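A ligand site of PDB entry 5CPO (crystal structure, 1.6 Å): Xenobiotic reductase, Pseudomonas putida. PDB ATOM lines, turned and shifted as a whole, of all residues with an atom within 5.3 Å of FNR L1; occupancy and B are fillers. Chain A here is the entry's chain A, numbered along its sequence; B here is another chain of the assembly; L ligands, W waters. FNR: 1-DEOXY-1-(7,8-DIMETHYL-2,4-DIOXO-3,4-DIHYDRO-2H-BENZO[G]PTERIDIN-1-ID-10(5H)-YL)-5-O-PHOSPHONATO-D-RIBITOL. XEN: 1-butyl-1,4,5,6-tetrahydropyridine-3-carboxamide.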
ATOM      1  N   PRO A  22      -3.820 -12.015  11.364  1.00  0.00           N
ATOM      2  CA  PRO A  22      -2.499 -11.372  11.327  1.00  0.00           C
ATOM      3  C   PRO A  22      -2.156 -10.815   9.974  1.00  0.00           C
ATOM      4  O   PRO A  22      -2.781 -11.219   8.962  1.00  0.00           O
ATOM      5  CB  PRO A  22      -1.549 -12.517  11.655  1.00  0.00           C
ATOM      6  CG  PRO A  22      -2.242 -13.721  11.017  1.00  0.00           C
ATOM      7  CD  PRO A  22      -3.722 -13.489  11.257  1.00  0.00           C
ATOM      8  N   PRO A  23      -1.161  -9.941   9.925  1.00  0.00           N
ATOM      9  CA  PRO A  23      -0.776  -9.405   8.618  1.00  0.00           C
ATOM     10  C   PRO A  23      -0.359 -10.517   7.648  1.00  0.00           C
ATOM     11  O   PRO A  23       0.406 -11.401   8.039  1.00  0.00           O
ATOM     12  CB  PRO A  23       0.398  -8.450   8.969  1.00  0.00           C
ATOM     13  CG  PRO A  23       0.971  -9.008  10.266  1.00  0.00           C
ATOM     14  CD  PRO A  23      -0.262  -9.471  11.005  1.00  0.00           C
ATOM     15  N   MET A  24      -0.920 -10.501   6.440  1.00  0.00           N
ATOM     16  CA  MET A  24      -0.498 -11.418   5.367  1.00  0.00           C
ATOM     17  C   MET A  24      -0.362 -10.708   4.036  1.00  0.00           C
ATOM     18  O   MET A  24      -1.361 -10.390   3.394  1.00  0.00           O
ATOM     19  CB  MET A  24      -1.499 -12.584   5.211  1.00  0.00           C
ATOM     20  CG  MET A  24      -1.478 -13.545   6.385  1.00  0.00           C
ATOM     21  SD  MET A  24      -2.702 -14.868   6.247  1.00  0.00           S
ATOM     22  CE  MET A  24      -4.210 -13.966   6.535  1.00  0.00           C
ATOM     23  N   CYS A  25       0.889 -10.451   3.641  1.00  0.00           N
ATOM     24  CA  CYS A  25       1.238  -9.903   2.316  1.00  0.00           C
ATOM     25  C   CYS A  25       0.490 -10.601   1.201  1.00  0.00           C
ATOM     26  O   CYS A  25       0.455 -11.827   1.146  1.00  0.00           O
ATOM     27  CB  CYS A  25       2.729 -10.062   2.043  1.00  0.00           C
ATOM     28  SG  CYS A  25       3.758  -8.921   2.987  1.00  0.00           S
ATOM     29  N   GLN A  26      -0.033  -9.783   0.301  1.00  0.00           N
ATOM     30  CA  GLN A  26      -0.813 -10.244  -0.845  1.00  0.00           C
ATOM     31  C   GLN A  26      -0.041 -10.140  -2.153  1.00  0.00           C
ATOM     32  O   GLN A  26      -0.399 -10.774  -3.145  1.00  0.00           O
ATOM     33  CB  GLN A  26      -2.111  -9.434  -0.927  1.00  0.00           C
ATOM     34  CG  GLN A  26      -3.049  -9.691   0.233  1.00  0.00           C
ATOM     35  CD  GLN A  26      -3.447 -11.139   0.310  1.00  0.00           C
ATOM     36  OE1 GLN A  26      -4.237 -11.639  -0.509  1.00  0.00           O
ATOM     37  NE2 GLN A  26      -2.860 -11.849   1.271  1.00  0.00           N
ATOM     38  N   TYR A  27       1.010  -9.322  -2.138  1.00  0.00           N
ATOM     39  CA  TYR A  27       1.875  -9.108  -3.311  1.00  0.00           C
ATOM     40  C   TYR A  27       1.103  -8.674  -4.569  1.00  0.00           C
ATOM     41  O   TYR A  27       1.505  -8.990  -5.696  1.00  0.00           O
ATOM     42  CB  TYR A  27       2.711 -10.367  -3.609  1.00  0.00           C
ATOM     43  CG  TYR A  27       3.410 -10.970  -2.401  1.00  0.00           C
ATOM     44  CD1 TYR A  27       4.678 -10.543  -2.013  1.00  0.00           C
ATOM     45  CD2 TYR A  27       2.800 -11.967  -1.648  1.00  0.00           C
ATOM     46  CE1 TYR A  27       5.310 -11.090  -0.916  1.00  0.00           C
ATOM     47  CE2 TYR A  27       3.424 -12.503  -0.550  1.00  0.00           C
ATOM     48  CZ  TYR A  27       4.686 -12.058  -0.194  1.00  0.00           C
ATOM     49  OH  TYR A  27       5.288 -12.583   0.905  1.00  0.00           O
ATOM     50  N   GLU A  56      -1.660  -6.360   6.027  1.00  0.00           N
ATOM     51  CA  GLU A  56      -0.326  -6.832   5.665  1.00  0.00           C
ATOM     52  C   GLU A  56       0.808  -5.817   5.836  1.00  0.00           C
ATOM     53  O   GLU A  56       0.587  -4.602   5.825  1.00  0.00           O
ATOM     54  CB  GLU A  56      -0.315  -7.242   4.204  1.00  0.00           C
ATOM     55  CG  GLU A  56      -0.533  -6.093   3.225  1.00  0.00           C
ATOM     56  CD  GLU A  56      -0.963  -6.580   1.838  1.00  0.00           C
ATOM     57  OE1 GLU A  56      -0.079  -6.896   0.998  1.00  0.00           O
ATOM     58  OE2 GLU A  56      -2.176  -6.657   1.611  1.00  0.00           O
ATOM     59  N   ALA A  57       2.029  -6.353   5.948  1.00  0.00           N
ATOM     60  CA  ALA A  57       3.243  -5.545   5.995  1.00  0.00           C
ATOM     61  C   ALA A  57       3.216  -4.453   4.917  1.00  0.00           C
ATOM     62  O   ALA A  57       3.187  -4.728   3.711  1.00  0.00           O
ATOM     63  CB  ALA A  57       4.481  -6.406   5.827  1.00  0.00           C
ATOM     64  N   GLN A  99       0.113  -3.298   9.931  1.00  0.00           N
ATOM     65  CA  GLN A  99       1.520  -3.520  10.206  1.00  0.00           C
ATOM     66  C   GLN A  99       2.405  -2.659   9.292  1.00  0.00           C
ATOM     67  O   GLN A  99       2.322  -2.784   8.059  1.00  0.00           O
ATOM     68  CB  GLN A  99       1.860  -5.001  10.031  1.00  0.00           C
ATOM     69  CG  GLN A  99       3.279  -5.329  10.434  1.00  0.00           C
ATOM     70  CD  GLN A  99       3.688  -6.725  10.027  1.00  0.00           C
ATOM     71  OE1 GLN A  99       3.692  -7.067   8.839  1.00  0.00           O
ATOM     72  NE2 GLN A  99       4.033  -7.554  11.019  1.00  0.00           N
ATOM     73  N   GLU A 176       0.894  -1.987  14.277  1.00  0.00           N
ATOM     74  CA  GLU A 176       1.867  -3.003  14.620  1.00  0.00           C
ATOM     75  C   GLU A 176       3.193  -2.684  13.941  1.00  0.00           C
ATOM     76  O   GLU A 176       3.261  -2.605  12.729  1.00  0.00           O
ATOM     77  CB  GLU A 176       1.378  -4.401  14.210  1.00  0.00           C
ATOM     78  CG  GLU A 176       2.291  -5.523  14.617  1.00  0.00           C
ATOM     79  CD  GLU A 176       1.776  -6.908  14.167  1.00  0.00           C
ATOM     80  OE1 GLU A 176       0.708  -7.361  14.642  1.00  0.00           O
ATOM     81  OE2 GLU A 176       2.453  -7.532  13.323  1.00  0.00           O
ATOM     82  N   HIS A 178       6.659  -3.756  12.602  1.00  0.00           N
ATOM     83  CA  HIS A 178       7.182  -5.047  12.170  1.00  0.00           C
ATOM     84  C   HIS A 178       8.667  -5.187  12.520  1.00  0.00           C
ATOM     85  O   HIS A 178       9.527  -4.806  11.739  1.00  0.00           O
ATOM     86  CB  HIS A 178       6.986  -5.240  10.656  1.00  0.00           C
ATOM     87  CG  HIS A 178       7.135  -6.653  10.216  1.00  0.00           C
ATOM     88  ND1 HIS A 178       7.615  -7.652  11.060  1.00  0.00           N
ATOM     89  CD2 HIS A 178       6.841  -7.267   9.043  1.00  0.00           C
ATOM     90  CE1 HIS A 178       7.603  -8.799  10.402  1.00  0.00           C
ATOM     91  NE2 HIS A 178       7.126  -8.596   9.183  1.00  0.00           N
ATOM     92  N   HIS A 181      10.817 -11.456  11.746  1.00  0.00           N
ATOM     93  CA  HIS A 181      10.984 -12.197  10.485  1.00  0.00           C
ATOM     94  C   HIS A 181      12.194 -11.799   9.655  1.00  0.00           C
ATOM     95  O   HIS A 181      12.216 -11.999   8.437  1.00  0.00           O
ATOM     96  CB  HIS A 181       9.695 -12.064   9.663  1.00  0.00           C
ATOM     97  CG  HIS A 181       8.491 -12.581  10.376  1.00  0.00           C
ATOM     98  ND1 HIS A 181       7.207 -12.377   9.928  1.00  0.00           N
ATOM     99  CD2 HIS A 181       8.377 -13.294  11.531  1.00  0.00           C
ATOM    100  CE1 HIS A 181       6.352 -12.949  10.772  1.00  0.00           C
ATOM    101  NE2 HIS A 181       7.046 -13.513  11.752  1.00  0.00           N
ATOM    102  N   ARG A 231       5.481  -6.650  16.403  1.00  0.00           N
ATOM    103  CA  ARG A 231       5.767  -8.060  16.198  1.00  0.00           C
ATOM    104  C   ARG A 231       7.272  -8.234  16.277  1.00  0.00           C
ATOM    105  O   ARG A 231       8.023  -7.430  15.737  1.00  0.00           O
ATOM    106  CB  ARG A 231       5.215  -8.562  14.840  1.00  0.00           C
ATOM    107  CG  ARG A 231       5.226 -10.088  14.722  1.00  0.00           C
ATOM    108  CD  ARG A 231       4.439 -10.592  13.532  1.00  0.00           C
ATOM    109  NE  ARG A 231       3.775 -11.858  13.868  1.00  0.00           N
ATOM    110  CZ  ARG A 231       3.003 -12.544  13.026  1.00  0.00           C
ATOM    111  NH1 ARG A 231       2.836 -12.110  11.773  1.00  0.00           N
ATOM    112  NH2 ARG A 231       2.420 -13.665  13.431  1.00  0.00           N
ATOM    113  N   ALA A 301       0.912 -16.885  16.433  1.00  0.00           N
ATOM    114  CA  ALA A 301       0.366 -17.561  15.272  1.00  0.00           C
ATOM    115  C   ALA A 301       1.152 -18.834  14.997  1.00  0.00           C
ATOM    116  O   ALA A 301       2.002 -19.221  15.792  1.00  0.00           O
ATOM    117  CB  ALA A 301       0.407 -16.631  14.072  1.00  0.00           C
ATOM    118  N   TRP A 302       1.018 -19.379  13.789  1.00  0.00           N
ATOM    119  CA  TRP A 302       1.855 -20.490  13.331  1.00  0.00           C
ATOM    120  C   TRP A 302       1.281 -21.784  13.887  1.00  0.00           C
ATOM    121  O   TRP A 302       1.903 -22.450  14.723  1.00  0.00           O
ATOM    122  CB  TRP A 302       3.338 -20.340  13.739  1.00  0.00           C
ATOM    123  CG  TRP A 302       4.006 -19.042  13.326  1.00  0.00           C
ATOM    124  CD1 TRP A 302       4.274 -17.941  14.122  1.00  0.00           C
ATOM    125  CD2 TRP A 302       4.493 -18.716  12.032  1.00  0.00           C
ATOM    126  NE1 TRP A 302       4.900 -16.980  13.387  1.00  0.00           N
ATOM    127  CE2 TRP A 302       5.042 -17.417  12.096  1.00  0.00           C
ATOM    128  CE3 TRP A 302       4.536 -19.396  10.821  1.00  0.00           C
ATOM    129  CZ2 TRP A 302       5.599 -16.795  11.006  1.00  0.00           C
ATOM    130  CZ3 TRP A 302       5.093 -18.765   9.727  1.00  0.00           C
ATOM    131  CH2 TRP A 302       5.626 -17.483   9.828  1.00  0.00           C
ATOM    132  N   GLY A 303       0.084 -22.132  13.424  1.00  0.00           N
ATOM    133  CA  GLY A 303      -0.576 -23.379  13.776  1.00  0.00           C
ATOM    134  C   GLY A 303      -1.741 -23.315  14.748  1.00  0.00           C
ATOM    135  O   GLY A 303      -1.775 -24.138  15.674  1.00  0.00           O
ATOM    136  N   PHE A 304      -2.707 -22.410  14.525  1.00  0.00           N
ATOM    137  CA  PHE A 304      -3.873 -22.244  15.405  1.00  0.00           C
ATOM    138  C   PHE A 304      -5.212 -22.268  14.678  1.00  0.00           C
ATOM    139  O   PHE A 304      -6.250 -22.006  15.297  1.00  0.00           O
ATOM    140  CB  PHE A 304      -3.789 -20.927  16.213  1.00  0.00           C
ATOM    141  CG  PHE A 304      -2.755 -20.932  17.296  1.00  0.00           C
ATOM    142  CD1 PHE A 304      -2.949 -21.637  18.477  1.00  0.00           C
ATOM    143  CD2 PHE A 304      -1.583 -20.207  17.165  1.00  0.00           C
ATOM    144  CE1 PHE A 304      -2.014 -21.647  19.464  1.00  0.00           C
ATOM    145  CE2 PHE A 304      -0.628 -20.194  18.152  1.00  0.00           C
ATOM    146  CZ  PHE A 304      -0.840 -20.928  19.320  1.00  0.00           C
ATOM    147  N   GLY A 305      -5.200 -22.596  13.376  1.00  0.00           N
ATOM    148  CA  GLY A 305      -6.407 -22.670  12.572  1.00  0.00           C
ATOM    149  C   GLY A 305      -7.304 -23.854  12.873  1.00  0.00           C
ATOM    150  O   GLY A 305      -8.242 -24.141  12.151  1.00  0.00           O
ATOM    151  N   SER A 323      -4.007 -15.476  16.667  1.00  0.00           N
ATOM    152  CA  SER A 323      -3.878 -15.025  15.272  1.00  0.00           C
ATOM    153  C   SER A 323      -3.970 -16.236  14.361  1.00  0.00           C
ATOM    154  O   SER A 323      -3.218 -17.205  14.492  1.00  0.00           O
ATOM    155  CB  SER A 323      -2.571 -14.275  15.037  1.00  0.00           C
ATOM    156  OG  SER A 323      -2.535 -13.039  15.744  1.00  0.00           O
ATOM    157  N   VAL A 324      -4.925 -16.162  13.444  1.00  0.00           N
ATOM    158  CA  VAL A 324      -5.248 -17.230  12.509  1.00  0.00           C
ATOM    159  C   VAL A 324      -5.123 -16.707  11.081  1.00  0.00           C
ATOM    160  O   VAL A 324      -5.927 -15.887  10.629  1.00  0.00           O
ATOM    161  CB  VAL A 324      -6.672 -17.756  12.793  1.00  0.00           C
ATOM    162  CG1 VAL A 324      -7.076 -18.830  11.804  1.00  0.00           C
ATOM    163  CG2 VAL A 324      -6.770 -18.280  14.240  1.00  0.00           C
ATOM    164  N   GLY A 325      -4.084 -17.149  10.380  1.00  0.00           N
ATOM    165  CA  GLY A 325      -3.737 -16.608   9.089  1.00  0.00           C
ATOM    166  C   GLY A 325      -4.225 -17.433   7.908  1.00  0.00           C
ATOM    167  O   GLY A 325      -5.254 -17.122   7.281  1.00  0.00           O
ATOM    168  N   ARG A 326      -3.476 -18.497   7.590  1.00  0.00           N
ATOM    169  CA  ARG A 326      -3.766 -19.280   6.384  1.00  0.00           C
ATOM    170  C   ARG A 326      -5.171 -19.857   6.334  1.00  0.00           C
ATOM    171  O   ARG A 326      -5.764 -19.936   5.258  1.00  0.00           O
ATOM    172  CB  ARG A 326      -2.721 -20.380   6.220  1.00  0.00           C
ATOM    173  CG  ARG A 326      -1.444 -19.875   5.592  1.00  0.00           C
ATOM    174  CD  ARG A 326      -0.261 -20.833   5.748  1.00  0.00           C
ATOM    175  NE  ARG A 326       0.096 -21.060   7.143  1.00  0.00           N
ATOM    176  CZ  ARG A 326       0.985 -21.969   7.537  1.00  0.00           C
ATOM    177  NH1 ARG A 326       1.600 -22.726   6.627  1.00  0.00           N
ATOM    178  NH2 ARG A 326       1.253 -22.140   8.825  1.00  0.00           N
ATOM    179  N   ALA A 327      -5.753 -20.188   7.485  1.00  0.00           N
ATOM    180  CA  ALA A 327      -7.117 -20.708   7.485  1.00  0.00           C
ATOM    181  C   ALA A 327      -8.120 -19.668   6.956  1.00  0.00           C
ATOM    182  O   ALA A 327      -9.195 -20.023   6.489  1.00  0.00           O
ATOM    183  CB  ALA A 327      -7.514 -21.176   8.870  1.00  0.00           C
ATOM    184  N   LEU A 329      -7.264 -17.453   4.549  1.00  0.00           N
ATOM    185  CA  LEU A 329      -7.035 -17.444   3.116  1.00  0.00           C
ATOM    186  C   LEU A 329      -7.898 -18.550   2.520  1.00  0.00           C
ATOM    187  O   LEU A 329      -8.520 -18.351   1.503  1.00  0.00           O
ATOM    188  CB  LEU A 329      -5.566 -17.677   2.756  1.00  0.00           C
ATOM    189  CG  LEU A 329      -4.558 -16.694   3.355  1.00  0.00           C
ATOM    190  CD1 LEU A 329      -3.161 -16.967   2.794  1.00  0.00           C
ATOM    191  CD2 LEU A 329      -4.966 -15.257   3.127  1.00  0.00           C
ATOM    192  N   PRO B 354      -2.388 -15.405  -4.719  1.00  0.00           N
ATOM    193  CA  PRO B 354      -2.017 -14.956  -3.361  1.00  0.00           C
ATOM    194  C   PRO B 354      -2.531 -15.850  -2.245  1.00  0.00           C
ATOM    195  O   PRO B 354      -2.107 -15.720  -1.088  1.00  0.00           O
ATOM    196  CB  PRO B 354      -2.643 -13.561  -3.246  1.00  0.00           C
ATOM    197  CG  PRO B 354      -2.836 -13.106  -4.714  1.00  0.00           C
ATOM    198  CD  PRO B 354      -3.165 -14.382  -5.455  1.00  0.00           C
ATOM    199  N   TRP B 358       0.145 -20.478  -0.966  1.00  0.00           N
ATOM    200  CA  TRP B 358       0.392 -20.752   0.435  1.00  0.00           C
ATOM    201  C   TRP B 358      -0.356 -21.973   0.952  1.00  0.00           C
ATOM    202  O   TRP B 358       0.018 -22.573   1.962  1.00  0.00           O
ATOM    203  CB  TRP B 358       0.026 -19.508   1.252  1.00  0.00           C
ATOM    204  CG  TRP B 358       0.854 -18.342   0.848  1.00  0.00           C
ATOM    205  CD1 TRP B 358       0.500 -17.321   0.011  1.00  0.00           C
ATOM    206  CD2 TRP B 358       2.206 -18.067   1.253  1.00  0.00           C
ATOM    207  NE1 TRP B 358       1.531 -16.442  -0.129  1.00  0.00           N
ATOM    208  CE2 TRP B 358       2.592 -16.856   0.634  1.00  0.00           C
ATOM    209  CE3 TRP B 358       3.126 -18.709   2.085  1.00  0.00           C
ATOM    210  CZ2 TRP B 358       3.847 -16.300   0.799  1.00  0.00           C
ATOM    211  CZ3 TRP B 358       4.370 -18.145   2.269  1.00  0.00           C
ATOM    212  CH2 TRP B 358       4.724 -16.946   1.628  1.00  0.00           C
HETATM  213  C9A FNR L   1       2.493 -14.190   6.196  1.00  0.00           C
HETATM  214  N10 FNR L   1       2.952 -13.723   7.511  1.00  0.00           N
HETATM  215  CAA FNR L   1       3.318 -12.318   7.683  1.00  0.00           C
HETATM  216  N1  FNR L   1       3.842 -11.946   8.830  1.00  0.00           N
HETATM  217  C2  FNR L   1       3.987 -10.637   9.104  1.00  0.00           C
HETATM  218  O2  FNR L   1       4.438 -10.317  10.171  1.00  0.00           O
HETATM  219  N3  FNR L   1       3.629  -9.719   8.164  1.00  0.00           N
HETATM  220  C4  FNR L   1       3.129 -10.076   6.975  1.00  0.00           C
HETATM  221  O4  FNR L   1       2.795  -9.239   6.168  1.00  0.00           O
HETATM  222  C4A FNR L   1       3.219 -11.417   6.651  1.00  0.00           C
HETATM  223  N5  FNR L   1       2.804 -11.917   5.357  1.00  0.00           N
HETATM  224  C5A FNR L   1       2.418 -13.305   5.151  1.00  0.00           C
HETATM  225  C6  FNR L   1       1.815 -13.698   3.941  1.00  0.00           C
HETATM  226  C7  FNR L   1       1.244 -14.948   3.845  1.00  0.00           C
HETATM  227  C7M FNR L   1       0.426 -15.199   2.584  1.00  0.00           C
HETATM  228  C8  FNR L   1       1.437 -15.858   4.870  1.00  0.00           C
HETATM  229  C8M FNR L   1       0.820 -17.256   4.788  1.00  0.00           C
HETATM  230  C9  FNR L   1       2.189 -15.525   5.977  1.00  0.00           C
HETATM  231  C1' FNR L   1       2.981 -14.655   8.650  1.00  0.00           C
HETATM  232  C2' FNR L   1       1.545 -14.743   9.196  1.00  0.00           C
HETATM  233  O2' FNR L   1       1.168 -13.504   9.739  1.00  0.00           O
HETATM  234  C3' FNR L   1       1.339 -15.835  10.252  1.00  0.00           C
HETATM  235  O3' FNR L   1       2.148 -15.616  11.394  1.00  0.00           O
HETATM  236  C4' FNR L   1       1.642 -17.217   9.646  1.00  0.00           C
HETATM  237  O4' FNR L   1       0.859 -17.388   8.486  1.00  0.00           O
HETATM  238  C5' FNR L   1       1.340 -18.320  10.664  1.00  0.00           C
HETATM  239  O5' FNR L   1      -0.008 -18.346  11.045  1.00  0.00           O
HETATM  240  P   FNR L   1      -1.027 -19.477  10.387  1.00  0.00           P
HETATM  241  O1P FNR L   1      -2.366 -19.288  11.024  1.00  0.00           O
HETATM  242  O2P FNR L   1      -0.501 -20.875  10.690  1.00  0.00           O
HETATM  243  O3P FNR L   1      -1.019 -19.239   8.878  1.00  0.00           O
HETATM  244  C1  XEN L   2       9.181 -14.929   7.241  1.00  0.00           C
HETATM  245  C2  XEN L   2       9.031 -16.389   7.019  1.00  0.00           C
HETATM  246  C3  XEN L   2       7.610 -16.836   6.604  1.00  0.00           C
HETATM  247  C4  XEN L   2       6.465 -15.901   7.024  1.00  0.00           C
HETATM  248  N5  XEN L   2       6.312 -14.785   6.060  1.00  0.00           N
HETATM  249  C6  XEN L   2       6.379 -13.553   6.585  1.00  0.00           C
HETATM  250  C7  XEN L   2       6.276 -12.435   5.790  1.00  0.00           C
HETATM  251  C8  XEN L   2       6.084 -12.565   4.413  1.00  0.00           C
HETATM  252  C9  XEN L   2       6.034 -13.889   3.877  1.00  0.00           C
HETATM  253  C10 XEN L   2       6.136 -14.984   4.747  1.00  0.00           C
HETATM  254  C11 XEN L   2       6.346 -11.063   6.455  1.00  0.00           C
HETATM  255  O12 XEN L   2       6.632 -10.943   7.654  1.00  0.00           O
HETATM  256  N13 XEN L   2       6.068  -9.911   5.584  1.00  0.00           N
HETATM  257  O   HOH W   1      -4.319 -20.762   9.982  1.00  0.00           O
HETATM  258  O   HOH W   2      -1.840 -23.036   9.689  1.00  0.00           O
HETATM  259  O   HOH W   3      -2.246 -19.596  13.696  1.00  0.00           O
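The side-chain amide oxygen (OE1) of Gln 99 lies within hydrogen-bond range of a nitrogen (N3) of FNR L1 (2.7 Å).
An oxygen (O3P) of FNR L1 is in hydrogen-bond range of the backbone NH (N) of Arg 326 (2.9 Å).
NE of Arg 326 is in salt-bridge range of O3P of FNR L1, 2.8 Å away.
An oxygen (O2') of FNR L1 lies within hydrogen-bond range of the backbone carbonyl oxygen (O) of Pro 23 (2.8 Å).
An oxygen (O1P) of FNR L1 sits at hydrogen-bond distance from the backbone NH of Gly 325 (2.8 Å).
NH2 of Arg 231 sits at hydrogen-bond distance from O3' of FNR L1, 2.8 Å away.
O4 of FNR L1 lies within hydrogen-bond range of N of Cys 25 (3.4 Å).
The side-chain sulfur (SG) of Cys 25 is in hydrogen-bond range of an oxygen (O4) of FNR L1 (3.3 Å).
An oxygen (O4) of FNR L1 sits at hydrogen-bond distance from the backbone NH of Ala 57 (3.0 Å).
The backbone NH (N) of Gly 303 lies within hydrogen-bond range of an oxygen (O2P) of FNR L1 (3.1 Å).
N of Trp 302 is in hydrogen-bond range of O5' of FNR L1, at 3.1 Å.
A ring nitrogen (ND1) of His 181 lies close to an oxygen (O2) of FNR L1.
An oxygen (O2) of FNR L1 lies within hydrogen-bond range of a ring nitrogen (NE2) of His 178, at 3.3 Å.
SG of Cys 25 lies within hydrogen-bond range of N13 of XEN L2 (3.6 Å).
ND1 of His 181 lies within hydrogen-bond range of O12 of XEN L2 (2.7 Å).
NE2 of His 178 sits at hydrogen-bond distance from O12 of XEN L2 (2.8 Å).
O12 of XEN L2 sits close to N1 of FNR L1, 3.2 Å away.
The backbone NH (N) of Ala 57 lies close to the side-chain amide oxygen (OE1) of Gln 99, 3.4 Å away.
The side-chain amide nitrogen of Gln 99 is in hydrogen-bond range of the side-chain carboxylate of Glu 176 (2.8 Å).
NE2 of Gln 26 lies within hydrogen-bond range of O of Met 24 (3.0 Å).
The side-chain carboxylate (OE1) of Glu 56 is in hydrogen-bond range of the backbone NH (N) of Gln 26, at 3.0 Å.
Residues that only touch FNR L1: Trp 358 of chain B, Met 24, Ala 301, Pro 22, Val 324 and Glu 56.
Hydrophobic or aromatic side chains that line FNR L1: Pro 22, Pro 23, Met 24, Ala 57, His 178, His 181, Ala 301, Trp 302 and Trp 358 of chain B.
17 residues have an atom within 4 Å of FNR L1: Pro 22, Pro 23, Met 24, Cys 25, Glu 56, Ala 57, Gln 99, His 178, His 181, Arg 231, Ala 301, Trp 302, Gly 303, Val 324, Gly 325, Arg 326 and Trp 358 of chain B.
Along chain A the residues within 4 Å of FNR L1 span positions 22 to 326.
The nearest printed residue that does not touch FNR L1 is Leu 329 (4.005 Å).
Water W1 lies within hydrogen-bond range of O1P of FNR L1, N of Ala 327 and N of Arg 326.
Water W2 bridges an oxygen (O2P) of FNR L1 (2.7 Å) and the guanidinium group of Arg 326 (3.3 Å).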
